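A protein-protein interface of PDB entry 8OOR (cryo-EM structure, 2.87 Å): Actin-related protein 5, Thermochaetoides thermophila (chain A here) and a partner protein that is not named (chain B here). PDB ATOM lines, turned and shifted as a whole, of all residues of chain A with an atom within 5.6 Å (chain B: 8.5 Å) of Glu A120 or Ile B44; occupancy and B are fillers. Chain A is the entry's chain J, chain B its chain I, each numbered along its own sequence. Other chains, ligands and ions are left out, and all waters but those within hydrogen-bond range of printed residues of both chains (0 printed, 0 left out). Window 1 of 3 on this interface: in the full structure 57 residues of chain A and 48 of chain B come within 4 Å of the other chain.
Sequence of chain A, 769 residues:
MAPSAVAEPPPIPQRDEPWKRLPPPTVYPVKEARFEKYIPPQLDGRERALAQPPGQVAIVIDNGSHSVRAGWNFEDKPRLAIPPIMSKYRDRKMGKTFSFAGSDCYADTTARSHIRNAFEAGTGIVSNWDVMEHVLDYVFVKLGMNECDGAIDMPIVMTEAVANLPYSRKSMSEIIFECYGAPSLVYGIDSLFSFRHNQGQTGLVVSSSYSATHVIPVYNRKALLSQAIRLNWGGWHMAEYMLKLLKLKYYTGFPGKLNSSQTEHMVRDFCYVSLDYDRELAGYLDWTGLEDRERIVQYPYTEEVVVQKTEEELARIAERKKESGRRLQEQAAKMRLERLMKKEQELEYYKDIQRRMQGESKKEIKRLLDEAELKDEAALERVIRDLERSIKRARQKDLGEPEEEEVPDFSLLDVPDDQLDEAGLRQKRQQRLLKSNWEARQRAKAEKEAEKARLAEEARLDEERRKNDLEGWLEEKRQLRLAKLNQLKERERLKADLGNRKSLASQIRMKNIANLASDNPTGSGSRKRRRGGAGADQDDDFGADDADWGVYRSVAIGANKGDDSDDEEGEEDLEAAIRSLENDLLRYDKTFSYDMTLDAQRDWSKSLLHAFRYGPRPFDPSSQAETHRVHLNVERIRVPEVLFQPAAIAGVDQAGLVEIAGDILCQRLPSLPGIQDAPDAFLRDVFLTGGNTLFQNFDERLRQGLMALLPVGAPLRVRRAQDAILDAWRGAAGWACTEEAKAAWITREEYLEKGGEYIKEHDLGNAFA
O of Lys B42 is in hydrogen-bond range of OG of Ser A127, at 3.3 Å.
The backbone NH (N) of Ile B44 sits close to the side-chain carboxylate (OE1) of Glu A120.
NZ of Lys B42 lies within salt-bridge range of OE1 of Glu B50.
N of Ala B46 lies within hydrogen-bond range of OG1 of Thr B43 (3.2 Å).
O of Ile B47 lies within hydrogen-bond range of OG of Ser B51, 3.0 Å away.
The backbone carbonyl oxygen (O) of Ala A118 lies within hydrogen-bond range of the backbone NH (N) of Ser A127 (2.7 Å).
N of Glu A120 lies within hydrogen-bond range of O of Ile A125, 3.3 Å away.
Among the printed residues, merely in contact across the chains: Ser A127 with Asn B41, Ile A125 with Ile B44, Leu A165 with Ile B47, Leu A165 with Ile B44, Leu A165 with Leu B48, Glu A120 with Thr B43 and Leu A165 with Asn B156.
Printed residues of chain B within 4 Å of Glu A120: Thr B43 and Ile B44.
No residue of chain B comes within 4 Å of Ala A121.
No residue of chain B comes within 4 Å of Thr A123.
Gly A124 touches none of the printed residues of chain B.
Printed residues of chain B within 4 Å of Ile A125: Ile B44.
Printed residues of chain B within 4 Å of Ser A127: Asn B41 (3.5 Å) and Lys B42 (3.3 Å).
Of the printed residues of chain B, Leu A165 touches Ile B44 (3.8 Å), Ile B47 (3.8 Å), Leu B48 (3.9 Å) and Asn B156 (3.9 Å).
Of the printed residues of chain A, Asn B41 touches Ser A127.
Ile B44 touches just these residues of chain A: Glu A120 (3.2 Å), Ile A125 (3.6 Å) and Leu A165 (3.8 Å).
Of the printed residues of chain A, Ile B47 touches Leu A165 (3.8 Å).
Glu B50 touches none of the printed residues of chain A.
The nearest residue of chain B that does not touch Glu A120 is Lys B45 (4.9 Å).
The nearest printed residue of chain B that does not touch Leu A165 is Ser B51 (6.0 Å).
Of the 12 printed residues of chain B, 7 touch a printed residue of chain A.
Printed residues of chain B that touch a printed residue of chain A: Asn B41, Lys B42, Thr B43, Ile B44, Ile B47, Leu B48 and Asn B156.
Hydrophobic or aromatic side chains of chain B that line the printed part of chain A: Ile B44, Ile B47 and Leu B48.
Among the printed residues, 9 pairs touch across the chains.
Among the printed residues, no Asp or Glu carboxylate lies within 4 Å of a Lys or Arg side-chain nitrogen of the other chain.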
ATOM      1  N   ASN A 117     -21.894 -28.075   0.011  1.00  0.00           N
ATOM      2  CA  ASN A 117     -21.840 -28.347  -1.416  1.00  0.00           C
ATOM      3  C   ASN A 117     -21.072 -27.241  -2.124  1.00  0.00           C
ATOM      4  O   ASN A 117     -21.177 -26.067  -1.759  1.00  0.00           O
ATOM      5  CB  ASN A 117     -23.268 -28.469  -1.965  1.00  0.00           C
ATOM      6  CG  ASN A 117     -23.318 -28.964  -3.380  1.00  0.00           C
ATOM      7  OD1 ASN A 117     -22.760 -28.358  -4.287  1.00  0.00           O
ATOM      8  ND2 ASN A 117     -23.972 -30.092  -3.574  1.00  0.00           N
ATOM      9  N   ALA A 118     -20.288 -27.628  -3.135  1.00  0.00           N
ATOM     10  CA  ALA A 118     -19.474 -26.663  -3.870  1.00  0.00           C
ATOM     11  C   ALA A 118     -20.304 -25.699  -4.707  1.00  0.00           C
ATOM     12  O   ALA A 118     -19.885 -24.560  -4.927  1.00  0.00           O
ATOM     13  CB  ALA A 118     -18.473 -27.399  -4.752  1.00  0.00           C
ATOM     14  N   PHE A 119     -21.450 -26.133  -5.207  1.00  0.00           N
ATOM     15  CA  PHE A 119     -22.254 -25.324  -6.109  1.00  0.00           C
ATOM     16  C   PHE A 119     -23.294 -24.521  -5.346  1.00  0.00           C
ATOM     17  O   PHE A 119     -23.761 -24.926  -4.280  1.00  0.00           O
ATOM     18  CB  PHE A 119     -22.915 -26.205  -7.160  1.00  0.00           C
ATOM     19  CG  PHE A 119     -21.940 -26.856  -8.077  1.00  0.00           C
ATOM     20  CD1 PHE A 119     -21.314 -28.028  -7.718  1.00  0.00           C
ATOM     21  CD2 PHE A 119     -21.645 -26.296  -9.299  1.00  0.00           C
ATOM     22  CE1 PHE A 119     -20.419 -28.623  -8.550  1.00  0.00           C
ATOM     23  CE2 PHE A 119     -20.755 -26.898 -10.139  1.00  0.00           C
ATOM     24  CZ  PHE A 119     -20.140 -28.060  -9.763  1.00  0.00           C
ATOM     25  N   GLU A 120     -23.653 -23.369  -5.901  1.00  0.00           N
ATOM     26  CA  GLU A 120     -24.837 -22.679  -5.426  1.00  0.00           C
ATOM     27  C   GLU A 120     -26.078 -23.507  -5.725  1.00  0.00           C
ATOM     28  O   GLU A 120     -26.132 -24.249  -6.704  1.00  0.00           O
ATOM     29  CB  GLU A 120     -24.945 -21.297  -6.061  1.00  0.00           C
ATOM     30  CG  GLU A 120     -26.163 -20.530  -5.613  1.00  0.00           C
ATOM     31  CD  GLU A 120     -25.984 -19.033  -5.685  1.00  0.00           C
ATOM     32  OE1 GLU A 120     -24.926 -18.546  -5.244  1.00  0.00           O
ATOM     33  OE2 GLU A 120     -26.914 -18.333  -6.130  1.00  0.00           O
ATOM     34  N   ALA A 121     -27.060 -23.417  -4.831  1.00  0.00           N
ATOM     35  CA  ALA A 121     -28.239 -24.270  -4.907  1.00  0.00           C
ATOM     36  C   ALA A 121     -28.940 -24.136  -6.250  1.00  0.00           C
ATOM     37  O   ALA A 121     -29.281 -23.032  -6.681  1.00  0.00           O
ATOM     38  CB  ALA A 121     -29.206 -23.922  -3.781  1.00  0.00           C
ATOM     39  N   GLY A 122     -29.190 -25.274  -6.888  1.00  0.00           N
ATOM     40  CA  GLY A 122     -29.870 -25.293  -8.164  1.00  0.00           C
ATOM     41  C   GLY A 122     -29.188 -24.559  -9.282  1.00  0.00           C
ATOM     42  O   GLY A 122     -29.850 -24.143 -10.230  1.00  0.00           O
ATOM     43  N   THR A 123     -27.891 -24.352  -9.185  1.00  0.00           N
ATOM     44  CA  THR A 123     -27.160 -23.494 -10.098  1.00  0.00           C
ATOM     45  C   THR A 123     -25.888 -24.205 -10.518  1.00  0.00           C
ATOM     46  O   THR A 123     -25.265 -24.896  -9.711  1.00  0.00           O
ATOM     47  CB  THR A 123     -26.852 -22.155  -9.465  1.00  0.00           C
ATOM     48  OG1 THR A 123     -28.077 -21.563  -9.035  1.00  0.00           O
ATOM     49  CG2 THR A 123     -26.226 -21.240 -10.462  1.00  0.00           C
ATOM     50  N   GLY A 124     -25.535 -24.079 -11.787  1.00  0.00           N
ATOM     51  CA  GLY A 124     -24.444 -24.832 -12.355  1.00  0.00           C
ATOM     52  C   GLY A 124     -23.078 -24.260 -12.077  1.00  0.00           C
ATOM     53  O   GLY A 124     -22.094 -24.726 -12.651  1.00  0.00           O
ATOM     54  N   ILE A 125     -22.986 -23.278 -11.191  1.00  0.00           N
ATOM     55  CA  ILE A 125     -21.787 -22.479 -10.988  1.00  0.00           C
ATOM     56  C   ILE A 125     -21.193 -22.829  -9.636  1.00  0.00           C
ATOM     57  O   ILE A 125     -21.921 -22.937  -8.643  1.00  0.00           O
ATOM     58  CB  ILE A 125     -22.106 -20.980 -11.068  1.00  0.00           C
ATOM     59  CG1 ILE A 125     -22.923 -20.692 -12.321  1.00  0.00           C
ATOM     60  CG2 ILE A 125     -20.845 -20.183 -11.086  1.00  0.00           C
ATOM     61  CD1 ILE A 125     -22.196 -20.966 -13.587  1.00  0.00           C
ATOM     62  N   VAL A 126     -19.878 -23.044  -9.599  1.00  0.00           N
ATOM     63  CA  VAL A 126     -19.198 -23.312  -8.339  1.00  0.00           C
ATOM     64  C   VAL A 126     -19.167 -22.048  -7.491  1.00  0.00           C
ATOM     65  O   VAL A 126     -18.985 -20.937  -8.002  1.00  0.00           O
ATOM     66  CB  VAL A 126     -17.783 -23.853  -8.586  1.00  0.00           C
ATOM     67  CG1 VAL A 126     -17.081 -24.081  -7.281  1.00  0.00           C
ATOM     68  CG2 VAL A 126     -17.849 -25.136  -9.352  1.00  0.00           C
ATOM     69  N   SER A 127     -19.368 -22.210  -6.185  1.00  0.00           N
ATOM     70  CA  SER A 127     -19.410 -21.068  -5.279  1.00  0.00           C
ATOM     71  C   SER A 127     -18.665 -21.267  -3.966  1.00  0.00           C
ATOM     72  O   SER A 127     -18.148 -20.286  -3.429  1.00  0.00           O
ATOM     73  CB  SER A 127     -20.865 -20.691  -4.977  1.00  0.00           C
ATOM     74  OG  SER A 127     -20.938 -19.717  -3.953  1.00  0.00           O
ATOM     75  N   LEU A 165     -19.381 -17.831 -15.125  1.00  0.00           N
ATOM     76  CA  LEU A 165     -19.068 -16.458 -14.775  1.00  0.00           C
ATOM     77  C   LEU A 165     -17.561 -16.232 -14.797  1.00  0.00           C
ATOM     78  O   LEU A 165     -16.797 -17.116 -14.403  1.00  0.00           O
ATOM     79  CB  LEU A 165     -19.630 -16.123 -13.402  1.00  0.00           C
ATOM     80  CG  LEU A 165     -21.141 -16.292 -13.322  1.00  0.00           C
ATOM     81  CD1 LEU A 165     -21.612 -16.031 -11.926  1.00  0.00           C
ATOM     82  CD2 LEU A 165     -21.775 -15.310 -14.273  1.00  0.00           C
ATOM     83  N   SER A 168     -15.802 -16.989 -11.634  1.00  0.00           N
ATOM     84  CA  SER A 168     -15.711 -18.411 -11.327  1.00  0.00           C
ATOM     85  C   SER A 168     -14.633 -19.087 -12.156  1.00  0.00           C
ATOM     86  O   SER A 168     -13.981 -20.026 -11.691  1.00  0.00           O
ATOM     87  CB  SER A 168     -17.061 -19.083 -11.537  1.00  0.00           C
ATOM     88  OG  SER A 168     -18.045 -18.432 -10.762  1.00  0.00           O
ATOM     89  N   ASN B  41     -15.621 -16.731  -1.501  1.00  0.00           N
ATOM     90  CA  ASN B  41     -16.894 -17.425  -1.654  1.00  0.00           C
ATOM     91  C   ASN B  41     -18.071 -16.482  -1.867  1.00  0.00           C
ATOM     92  O   ASN B  41     -19.076 -16.571  -1.161  1.00  0.00           O
ATOM     93  CB  ASN B  41     -17.171 -18.298  -0.438  1.00  0.00           C
ATOM     94  CG  ASN B  41     -16.332 -19.536  -0.426  1.00  0.00           C
ATOM     95  OD1 ASN B  41     -15.451 -19.704  -1.259  1.00  0.00           O
ATOM     96  ND2 ASN B  41     -16.606 -20.424   0.511  1.00  0.00           N
ATOM     97  N   LYS B  42     -17.963 -15.591  -2.842  1.00  0.00           N
ATOM     98  CA  LYS B  42     -19.070 -14.721  -3.214  1.00  0.00           C
ATOM     99  C   LYS B  42     -20.242 -15.527  -3.766  1.00  0.00           C
ATOM    100  O   LYS B  42     -20.067 -16.591  -4.363  1.00  0.00           O
ATOM    101  CB  LYS B  42     -18.588 -13.714  -4.246  1.00  0.00           C
ATOM    102  CG  LYS B  42     -17.766 -12.601  -3.657  1.00  0.00           C
ATOM    103  CD  LYS B  42     -16.671 -12.190  -4.606  1.00  0.00           C
ATOM    104  CE  LYS B  42     -17.180 -12.079  -6.019  1.00  0.00           C
ATOM    105  NZ  LYS B  42     -16.182 -11.404  -6.884  1.00  0.00           N
ATOM    106  N   THR B  43     -21.454 -15.020  -3.542  1.00  0.00           N
ATOM    107  CA  THR B  43     -22.656 -15.578  -4.147  1.00  0.00           C
ATOM    108  C   THR B  43     -22.803 -15.129  -5.597  1.00  0.00           C
ATOM    109  O   THR B  43     -22.209 -14.142  -6.034  1.00  0.00           O
ATOM    110  CB  THR B  43     -23.907 -15.176  -3.372  1.00  0.00           C
ATOM    111  OG1 THR B  43     -24.100 -13.763  -3.476  1.00  0.00           O
ATOM    112  CG2 THR B  43     -23.776 -15.565  -1.920  1.00  0.00           C
ATOM    113  N   ILE B  44     -23.647 -15.856  -6.333  1.00  0.00           N
ATOM    114  CA  ILE B  44     -23.926 -15.512  -7.726  1.00  0.00           C
ATOM    115  C   ILE B  44     -24.519 -14.115  -7.841  1.00  0.00           C
ATOM    116  O   ILE B  44     -24.192 -13.368  -8.768  1.00  0.00           O
ATOM    117  CB  ILE B  44     -24.867 -16.558  -8.349  1.00  0.00           C
ATOM    118  CG1 ILE B  44     -24.240 -17.947  -8.282  1.00  0.00           C
ATOM    119  CG2 ILE B  44     -25.198 -16.191  -9.776  1.00  0.00           C
ATOM    120  CD1 ILE B  44     -22.969 -18.066  -9.028  1.00  0.00           C
ATOM    121  N   LYS B  45     -25.404 -13.741  -6.919  1.00  0.00           N
ATOM    122  CA  LYS B  45     -25.918 -12.375  -6.921  1.00  0.00           C
ATOM    123  C   LYS B  45     -24.803 -11.358  -6.740  1.00  0.00           C
ATOM    124  O   LYS B  45     -24.777 -10.326  -7.418  1.00  0.00           O
ATOM    125  CB  LYS B  45     -26.967 -12.188  -5.828  1.00  0.00           C
ATOM    126  CG  LYS B  45     -27.632 -10.821  -5.897  1.00  0.00           C
ATOM    127  CD  LYS B  45     -28.616 -10.589  -4.767  1.00  0.00           C
ATOM    128  CE  LYS B  45     -29.771 -11.560  -4.827  1.00  0.00           C
ATOM    129  NZ  LYS B  45     -30.673 -11.285  -5.981  1.00  0.00           N
ATOM    130  N   ALA B  46     -23.877 -11.629  -5.822  1.00  0.00           N
ATOM    131  CA  ALA B  46     -22.746 -10.733  -5.616  1.00  0.00           C
ATOM    132  C   ALA B  46     -21.844 -10.671  -6.839  1.00  0.00           C
ATOM    133  O   ALA B  46     -21.420  -9.586  -7.252  1.00  0.00           O
ATOM    134  CB  ALA B  46     -21.951 -11.175  -4.391  1.00  0.00           C
ATOM    135  N   ILE B  47     -21.549 -11.822  -7.441  1.00  0.00           N
ATOM    136  CA  ILE B  47     -20.689 -11.845  -8.618  1.00  0.00           C
ATOM    137  C   ILE B  47     -21.306 -11.052  -9.761  1.00  0.00           C
ATOM    138  O   ILE B  47     -20.616 -10.288 -10.445  1.00  0.00           O
ATOM    139  CB  ILE B  47     -20.394 -13.294  -9.031  1.00  0.00           C
ATOM    140  CG1 ILE B  47     -19.605 -14.000  -7.941  1.00  0.00           C
ATOM    141  CG2 ILE B  47     -19.583 -13.307 -10.282  1.00  0.00           C
ATOM    142  CD1 ILE B  47     -19.706 -15.486  -8.002  1.00  0.00           C
ATOM    143  N   LEU B  48     -22.610 -11.203  -9.981  1.00  0.00           N
ATOM    144  CA  LEU B  48     -23.283 -10.380 -10.980  1.00  0.00           C
ATOM    145  C   LEU B  48     -23.238  -8.904 -10.612  1.00  0.00           C
ATOM    146  O   LEU B  48     -23.026  -8.048 -11.477  1.00  0.00           O
ATOM    147  CB  LEU B  48     -24.726 -10.839 -11.165  1.00  0.00           C
ATOM    148  CG  LEU B  48     -24.996 -11.834 -12.292  1.00  0.00           C
ATOM    149  CD1 LEU B  48     -24.749 -11.144 -13.617  1.00  0.00           C
ATOM    150  CD2 LEU B  48     -24.149 -13.082 -12.180  1.00  0.00           C
ATOM    151  N   GLY B  49     -23.448  -8.586  -9.337  1.00  0.00           N
ATOM    152  CA  GLY B  49     -23.367  -7.202  -8.899  1.00  0.00           C
ATOM    153  C   GLY B  49     -21.989  -6.600  -9.094  1.00  0.00           C
ATOM    154  O   GLY B  49     -21.857  -5.430  -9.456  1.00  0.00           O
ATOM    155  N   GLU B  50     -20.946  -7.389  -8.845  1.00  0.00           N
ATOM    156  CA  GLU B  50     -19.583  -6.950  -9.111  1.00  0.00           C
ATOM    157  C   GLU B  50     -19.275  -6.841 -10.596  1.00  0.00           C
ATOM    158  O   GLU B  50     -18.342  -6.125 -10.969  1.00  0.00           O
ATOM    159  CB  GLU B  50     -18.606  -7.907  -8.438  1.00  0.00           C
ATOM    160  CG  GLU B  50     -18.630  -7.790  -6.934  1.00  0.00           C
ATOM    161  CD  GLU B  50     -17.703  -8.767  -6.260  1.00  0.00           C
ATOM    162  OE1 GLU B  50     -16.584  -8.978  -6.772  1.00  0.00           O
ATOM    163  OE2 GLU B  50     -18.090  -9.315  -5.206  1.00  0.00           O
ATOM    164  N   SER B  51     -20.026  -7.523 -11.451  1.00  0.00           N
ATOM    165  CA  SER B  51     -19.936  -7.264 -12.880  1.00  0.00           C
ATOM    166  C   SER B  51     -20.659  -5.985 -13.280  1.00  0.00           C
ATOM    167  O   SER B  51     -20.709  -5.665 -14.471  1.00  0.00           O
ATOM    168  CB  SER B  51     -20.493  -8.448 -13.676  1.00  0.00           C
ATOM    169  OG  SER B  51     -19.897  -9.669 -13.274  1.00  0.00           O
ATOM    170  N   ASN B 156     -24.710 -15.638 -19.100  1.00  0.00           N
ATOM    171  CA  ASN B 156     -25.581 -16.011 -17.987  1.00  0.00           C
ATOM    172  C   ASN B 156     -26.878 -15.201 -17.988  1.00  0.00           C
ATOM    173  O   ASN B 156     -27.446 -14.927 -16.934  1.00  0.00           O
ATOM    174  CB  ASN B 156     -24.860 -15.887 -16.640  1.00  0.00           C
ATOM    175  CG  ASN B 156     -25.349 -16.895 -15.615  1.00  0.00           C
ATOM    176  OD1 ASN B 156     -24.888 -18.030 -15.582  1.00  0.00           O
ATOM    177  ND2 ASN B 156     -26.293 -16.485 -14.780  1.00  0.00           N
